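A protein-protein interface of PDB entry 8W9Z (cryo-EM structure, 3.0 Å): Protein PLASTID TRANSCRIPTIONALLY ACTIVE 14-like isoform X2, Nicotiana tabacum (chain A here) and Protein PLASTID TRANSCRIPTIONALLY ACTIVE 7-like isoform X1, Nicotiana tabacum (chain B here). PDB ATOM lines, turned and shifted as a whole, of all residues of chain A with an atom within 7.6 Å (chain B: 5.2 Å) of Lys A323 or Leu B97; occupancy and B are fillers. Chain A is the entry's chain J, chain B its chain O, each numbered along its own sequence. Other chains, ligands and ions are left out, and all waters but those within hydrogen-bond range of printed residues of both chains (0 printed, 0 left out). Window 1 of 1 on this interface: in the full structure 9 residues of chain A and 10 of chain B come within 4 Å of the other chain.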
ATOM      1  N   GLU A 144      -0.030  33.026  23.855  1.00  0.00           N
ATOM      2  CA  GLU A 144       0.876  32.248  23.013  1.00  0.00           C
ATOM      3  C   GLU A 144       2.249  32.906  23.105  1.00  0.00           C
ATOM      4  O   GLU A 144       2.494  33.938  22.473  1.00  0.00           O
ATOM      5  CB  GLU A 144       0.381  32.180  21.572  1.00  0.00           C
ATOM      6  CG  GLU A 144      -0.925  31.425  21.399  1.00  0.00           C
ATOM      7  CD  GLU A 144      -1.364  31.345  19.951  1.00  0.00           C
ATOM      8  OE1 GLU A 144      -0.658  31.901  19.083  1.00  0.00           O
ATOM      9  OE2 GLU A 144      -2.414  30.727  19.680  1.00  0.00           O
ATOM     10  N   ARG A 290       9.303  19.829  25.003  1.00  0.00           N
ATOM     11  CA  ARG A 290       9.785  18.955  23.941  1.00  0.00           C
ATOM     12  C   ARG A 290      10.097  19.793  22.713  1.00  0.00           C
ATOM     13  O   ARG A 290       9.224  20.506  22.208  1.00  0.00           O
ATOM     14  CB  ARG A 290       8.755  17.878  23.597  1.00  0.00           C
ATOM     15  CG  ARG A 290       9.076  17.122  22.322  1.00  0.00           C
ATOM     16  CD  ARG A 290       7.939  16.207  21.913  1.00  0.00           C
ATOM     17  NE  ARG A 290       8.141  15.662  20.574  1.00  0.00           N
ATOM     18  CZ  ARG A 290       7.249  14.919  19.928  1.00  0.00           C
ATOM     19  NH1 ARG A 290       6.087  14.629  20.495  1.00  0.00           N
ATOM     20  NH2 ARG A 290       7.518  14.468  18.711  1.00  0.00           N
ATOM     21  N   HIS A 319       0.504  25.009  29.126  1.00  0.00           N
ATOM     22  CA  HIS A 319       0.592  23.891  28.200  1.00  0.00           C
ATOM     23  C   HIS A 319       1.671  24.180  27.169  1.00  0.00           C
ATOM     24  O   HIS A 319       1.785  25.306  26.676  1.00  0.00           O
ATOM     25  CB  HIS A 319      -0.747  23.637  27.502  1.00  0.00           C
ATOM     26  CG  HIS A 319      -0.752  22.424  26.626  1.00  0.00           C
ATOM     27  ND1 HIS A 319      -0.381  21.177  27.080  1.00  0.00           N
ATOM     28  CD2 HIS A 319      -1.086  22.265  25.323  1.00  0.00           C
ATOM     29  CE1 HIS A 319      -0.485  20.303  26.096  1.00  0.00           C
ATOM     30  NE2 HIS A 319      -0.911  20.938  25.019  1.00  0.00           N
ATOM     31  N   TRP A 320       2.461  23.161  26.846  1.00  0.00           N
ATOM     32  CA  TRP A 320       3.560  23.291  25.900  1.00  0.00           C
ATOM     33  C   TRP A 320       3.132  22.739  24.546  1.00  0.00           C
ATOM     34  O   TRP A 320       2.711  21.582  24.447  1.00  0.00           O
ATOM     35  CB  TRP A 320       4.804  22.564  26.408  1.00  0.00           C
ATOM     36  CG  TRP A 320       5.946  22.622  25.449  1.00  0.00           C
ATOM     37  CD1 TRP A 320       6.319  21.659  24.561  1.00  0.00           C
ATOM     38  CD2 TRP A 320       6.859  23.709  25.271  1.00  0.00           C
ATOM     39  NE1 TRP A 320       7.413  22.077  23.843  1.00  0.00           N
ATOM     40  CE2 TRP A 320       7.763  23.334  24.259  1.00  0.00           C
ATOM     41  CE3 TRP A 320       7.001  24.964  25.869  1.00  0.00           C
ATOM     42  CZ2 TRP A 320       8.794  24.165  23.835  1.00  0.00           C
ATOM     43  CZ3 TRP A 320       8.023  25.787  25.446  1.00  0.00           C
ATOM     44  CH2 TRP A 320       8.906  25.386  24.439  1.00  0.00           C
ATOM     45  N   ARG A 321       3.243  23.566  23.510  1.00  0.00           N
ATOM     46  CA  ARG A 321       2.957  23.165  22.138  1.00  0.00           C
ATOM     47  C   ARG A 321       4.285  22.960  21.419  1.00  0.00           C
ATOM     48  O   ARG A 321       5.049  23.912  21.230  1.00  0.00           O
ATOM     49  CB  ARG A 321       2.104  24.215  21.429  1.00  0.00           C
ATOM     50  CG  ARG A 321       1.711  23.836  20.015  1.00  0.00           C
ATOM     51  CD  ARG A 321       1.256  25.046  19.216  1.00  0.00           C
ATOM     52  NE  ARG A 321       0.133  25.737  19.840  1.00  0.00           N
ATOM     53  CZ  ARG A 321      -0.499  26.773  19.298  1.00  0.00           C
ATOM     54  NH1 ARG A 321      -0.120  27.239  18.117  1.00  0.00           N
ATOM     55  NH2 ARG A 321      -1.512  27.342  19.936  1.00  0.00           N
ATOM     56  N   PHE A 322       4.560  21.719  21.020  1.00  0.00           N
ATOM     57  CA  PHE A 322       5.844  21.381  20.419  1.00  0.00           C
ATOM     58  C   PHE A 322       5.886  21.606  18.914  1.00  0.00           C
ATOM     59  O   PHE A 322       6.981  21.657  18.344  1.00  0.00           O
ATOM     60  CB  PHE A 322       6.203  19.923  20.723  1.00  0.00           C
ATOM     61  CG  PHE A 322       5.292  18.922  20.069  1.00  0.00           C
ATOM     62  CD1 PHE A 322       4.074  18.596  20.642  1.00  0.00           C
ATOM     63  CD2 PHE A 322       5.658  18.300  18.889  1.00  0.00           C
ATOM     64  CE1 PHE A 322       3.236  17.676  20.045  1.00  0.00           C
ATOM     65  CE2 PHE A 322       4.825  17.378  18.287  1.00  0.00           C
ATOM     66  CZ  PHE A 322       3.612  17.065  18.867  1.00  0.00           C
ATOM     67  N   LYS A 323       4.730  21.733  18.258  1.00  0.00           N
ATOM     68  CA  LYS A 323       4.724  21.952  16.816  1.00  0.00           C
ATOM     69  C   LYS A 323       5.216  23.346  16.454  1.00  0.00           C
ATOM     70  O   LYS A 323       5.826  23.530  15.395  1.00  0.00           O
ATOM     71  CB  LYS A 323       3.321  21.726  16.253  1.00  0.00           C
ATOM     72  CG  LYS A 323       2.900  20.268  16.201  1.00  0.00           C
ATOM     73  CD  LYS A 323       3.751  19.487  15.215  1.00  0.00           C
ATOM     74  CE  LYS A 323       3.272  18.050  15.089  1.00  0.00           C
ATOM     75  NZ  LYS A 323       4.100  17.270  14.127  1.00  0.00           N
ATOM     76  N   ASP A 324       4.966  24.333  17.312  1.00  0.00           N
ATOM     77  CA  ASP A 324       5.412  25.698  17.077  1.00  0.00           C
ATOM     78  C   ASP A 324       6.371  26.204  18.143  1.00  0.00           C
ATOM     79  O   ASP A 324       6.820  27.353  18.050  1.00  0.00           O
ATOM     80  CB  ASP A 324       4.208  26.645  16.989  1.00  0.00           C
ATOM     81  CG  ASP A 324       3.268  26.289  15.857  1.00  0.00           C
ATOM     82  OD1 ASP A 324       3.740  25.737  14.841  1.00  0.00           O
ATOM     83  OD2 ASP A 324       2.057  26.564  15.984  1.00  0.00           O
ATOM     84  N   ARG A 325       6.698  25.385  19.141  1.00  0.00           N
ATOM     85  CA  ARG A 325       7.572  25.779  20.244  1.00  0.00           C
ATOM     86  C   ARG A 325       7.053  27.040  20.930  1.00  0.00           C
ATOM     87  O   ARG A 325       7.761  28.039  21.077  1.00  0.00           O
ATOM     88  CB  ARG A 325       9.014  25.956  19.768  1.00  0.00           C
ATOM     89  CG  ARG A 325       9.701  24.653  19.394  1.00  0.00           C
ATOM     90  CD  ARG A 325      11.202  24.838  19.254  1.00  0.00           C
ATOM     91  NE  ARG A 325      11.622  24.957  17.863  1.00  0.00           N
ATOM     92  CZ  ARG A 325      12.100  23.950  17.141  1.00  0.00           C
ATOM     93  NH1 ARG A 325      12.220  22.744  17.681  1.00  0.00           N
ATOM     94  NH2 ARG A 325      12.459  24.144  15.880  1.00  0.00           N
ATOM     95  N   MET A 326       5.792  26.984  21.355  1.00  0.00           N
ATOM     96  CA  MET A 326       5.145  28.086  22.051  1.00  0.00           C
ATOM     97  C   MET A 326       4.432  27.560  23.286  1.00  0.00           C
ATOM     98  O   MET A 326       3.792  26.506  23.243  1.00  0.00           O
ATOM     99  CB  MET A 326       4.143  28.811  21.146  1.00  0.00           C
ATOM    100  CG  MET A 326       4.770  29.528  19.963  1.00  0.00           C
ATOM    101  SD  MET A 326       3.608  30.610  19.109  1.00  0.00           S
ATOM    102  CE  MET A 326       2.348  29.436  18.622  1.00  0.00           C
ATOM    103  N   GLU A 328       1.478  27.895  26.113  1.00  0.00           N
ATOM    104  CA  GLU A 328       0.096  28.346  26.105  1.00  0.00           C
ATOM    105  C   GLU A 328      -0.444  28.418  27.525  1.00  0.00           C
ATOM    106  O   GLU A 328      -0.076  27.609  28.382  1.00  0.00           O
ATOM    107  CB  GLU A 328      -0.787  27.413  25.275  1.00  0.00           C
ATOM    108  CG  GLU A 328      -0.322  27.210  23.850  1.00  0.00           C
ATOM    109  CD  GLU A 328      -1.179  26.206  23.108  1.00  0.00           C
ATOM    110  OE1 GLU A 328      -2.314  25.946  23.558  1.00  0.00           O
ATOM    111  OE2 GLU A 328      -0.717  25.671  22.080  1.00  0.00           O
ATOM    112  N   HIS B  93      -4.867  23.308   9.356  1.00  0.00           N
ATOM    113  CA  HIS B  93      -3.463  23.418   9.732  1.00  0.00           C
ATOM    114  C   HIS B  93      -3.301  23.941  11.153  1.00  0.00           C
ATOM    115  O   HIS B  93      -2.350  23.562  11.845  1.00  0.00           O
ATOM    116  CB  HIS B  93      -2.723  24.320   8.744  1.00  0.00           C
ATOM    117  CG  HIS B  93      -1.253  24.423   9.005  1.00  0.00           C
ATOM    118  ND1 HIS B  93      -0.702  25.418   9.783  1.00  0.00           N
ATOM    119  CD2 HIS B  93      -0.218  23.655   8.589  1.00  0.00           C
ATOM    120  CE1 HIS B  93       0.608  25.259   9.835  1.00  0.00           C
ATOM    121  NE2 HIS B  93       0.928  24.196   9.120  1.00  0.00           N
ATOM    122  N   ARG B  94      -4.210  24.808  11.605  1.00  0.00           N
ATOM    123  CA  ARG B  94      -4.139  25.294  12.978  1.00  0.00           C
ATOM    124  C   ARG B  94      -4.519  24.200  13.969  1.00  0.00           C
ATOM    125  O   ARG B  94      -3.912  24.088  15.040  1.00  0.00           O
ATOM    126  CB  ARG B  94      -5.037  26.519  13.150  1.00  0.00           C
ATOM    127  N   LEU B  95      -5.523  23.387  13.631  1.00  0.00           N
ATOM    128  CA  LEU B  95      -5.918  22.296  14.511  1.00  0.00           C
ATOM    129  C   LEU B  95      -4.886  21.177  14.543  1.00  0.00           C
ATOM    130  O   LEU B  95      -4.787  20.475  15.553  1.00  0.00           O
ATOM    131  CB  LEU B  95      -7.278  21.740  14.088  1.00  0.00           C
ATOM    132  CG  LEU B  95      -8.480  22.667  14.272  1.00  0.00           C
ATOM    133  CD1 LEU B  95      -9.758  21.977  13.832  1.00  0.00           C
ATOM    134  CD2 LEU B  95      -8.587  23.127  15.716  1.00  0.00           C
ATOM    135  N   LEU B  96      -4.119  20.997  13.470  1.00  0.00           N
ATOM    136  CA  LEU B  96      -3.055  20.001  13.460  1.00  0.00           C
ATOM    137  C   LEU B  96      -1.798  20.460  14.193  1.00  0.00           C
ATOM    138  O   LEU B  96      -0.767  19.786  14.100  1.00  0.00           O
ATOM    139  CB  LEU B  96      -2.699  19.619  12.020  1.00  0.00           C
ATOM    140  CG  LEU B  96      -3.676  18.695  11.293  1.00  0.00           C
ATOM    141  CD1 LEU B  96      -3.219  18.446   9.865  1.00  0.00           C
ATOM    142  CD2 LEU B  96      -3.826  17.385  12.044  1.00  0.00           C
ATOM    143  N   LEU B  97      -1.854  21.580  14.912  1.00  0.00           N
ATOM    144  CA  LEU B  97      -0.710  22.082  15.662  1.00  0.00           C
ATOM    145  C   LEU B  97      -0.701  21.632  17.117  1.00  0.00           C
ATOM    146  O   LEU B  97       0.309  21.827  17.800  1.00  0.00           O
ATOM    147  CB  LEU B  97      -0.669  23.614  15.610  1.00  0.00           C
ATOM    148  CG  LEU B  97      -0.330  24.253  14.262  1.00  0.00           C
ATOM    149  CD1 LEU B  97      -0.577  25.752  14.303  1.00  0.00           C
ATOM    150  CD2 LEU B  97       1.110  23.956  13.878  1.00  0.00           C
ATOM    151  N   ASN B  98      -1.790  21.040  17.605  1.00  0.00           N
ATOM    152  CA  ASN B  98      -1.863  20.569  18.979  1.00  0.00           C
ATOM    153  C   ASN B  98      -1.827  19.053  19.099  1.00  0.00           C
ATOM    154  O   ASN B  98      -1.652  18.542  20.211  1.00  0.00           O
ATOM    155  CB  ASN B  98      -3.140  21.094  19.654  1.00  0.00           C
ATOM    156  CG  ASN B  98      -3.251  22.603  19.599  1.00  0.00           C
ATOM    157  OD1 ASN B  98      -4.209  23.147  19.052  1.00  0.00           O
ATOM    158  ND2 ASN B  98      -2.267  23.290  20.168  1.00  0.00           N
ATOM    159  N   GLU B  99      -1.985  18.327  17.997  1.00  0.00           N
ATOM    160  CA  GLU B  99      -2.022  16.872  18.002  1.00  0.00           C
ATOM    161  C   GLU B  99      -0.685  16.315  17.537  1.00  0.00           C
ATOM    162  O   GLU B  99      -0.063  16.855  16.617  1.00  0.00           O
ATOM    163  CB  GLU B  99      -3.145  16.349  17.103  1.00  0.00           C
ATOM    164  CG  GLU B  99      -4.528  16.324  17.747  1.00  0.00           C
ATOM    165  CD  GLU B  99      -5.020  17.698  18.164  1.00  0.00           C
ATOM    166  OE1 GLU B  99      -4.708  18.128  19.294  1.00  0.00           O
ATOM    167  OE2 GLU B  99      -5.719  18.349  17.360  1.00  0.00           O
ATOM    168  N   ASP B 100      -0.248  15.230  18.177  1.00  0.00           N
ATOM    169  CA  ASP B 100       0.994  14.581  17.773  1.00  0.00           C
ATOM    170  C   ASP B 100       0.813  13.835  16.457  1.00  0.00           C
ATOM    171  O   ASP B 100       1.451  14.159  15.450  1.00  0.00           O
ATOM    172  CB  ASP B 100       1.470  13.633  18.874  1.00  0.00           C
ATOM    173  CG  ASP B 100       2.862  13.089  18.618  1.00  0.00           C
ATOM    174  OD1 ASP B 100       3.537  13.584  17.690  1.00  0.00           O
ATOM    175  OD2 ASP B 100       3.281  12.164  19.345  1.00  0.00           O
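OD2 of Asp B100 lies within salt-bridge range of NH1 of Arg A290 (3.9 Å).
OE2 of Glu A328 lies within hydrogen-bond range of ND2 of Asn B98 (3.4 Å).
The guanidinium group (NE) of Arg A321 sits close to the side-chain amide nitrogen (ND2) of Asn B98.
O of Arg A290 sits at hydrogen-bond distance from NE1 of Trp A320, at 2.9 Å.
O of Met A326 sits at hydrogen-bond distance from N of Arg A321 (3.0 Å).
N of Glu A328 lies within hydrogen-bond range of O of His A319, 2.7 Å away.
The guanidinium group (NH1) of Arg A321 lies within salt-bridge range of the side-chain carboxylate (OD2) of Asp A324 (3.1 Å).
The guanidinium group (NH2) of Arg A321 lies within salt-bridge range of the side-chain carboxylate (OE2) of Glu A328, 2.8 Å away.
The guanidinium group (NH2) of Arg A321 is in salt-bridge range of the side-chain carboxylate (OE2) of Glu A144 (3.5 Å).
CG of Arg A321 touches O of Leu B97 (3.3 Å).
Phe A322 touches Asp B100 (CZ to OD1, 3.7 Å).
Lys A323 touches Leu B97.
O of Glu B99 touches CE of Lys A323, 3.9 Å away.
OD2 of Asp A324 touches CD1 of Leu B97, at 3.2 Å.
Of the 8 printed residues of chain B, 4 touch a printed residue of chain A.
Among the printed residues, 8 pairs touch across the chains.
Lys A323 touches just these residues of chain B: Leu B97 and Glu B99.
Printed residues of chain A within 4 Å of Leu B97: Arg A321 (3.3 Å), Lys A323 (3.4 Å) and Asp A324 (3.2 Å).
Of the printed residues of chain B, Arg A290 touches Asp B100 (3.9 Å).
Of the printed residues of chain A, Asp B100 touches Arg A290 (3.9 Å) and Phe A322 (3.7 Å).
Arg A325 touches none of the printed residues of chain B.
The nearest residue of chain B that does not touch Lys A323 is Leu B96 (4.3 Å).
The nearest residue of chain A that does not touch Leu B97 is Phe A322 (5.3 Å).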
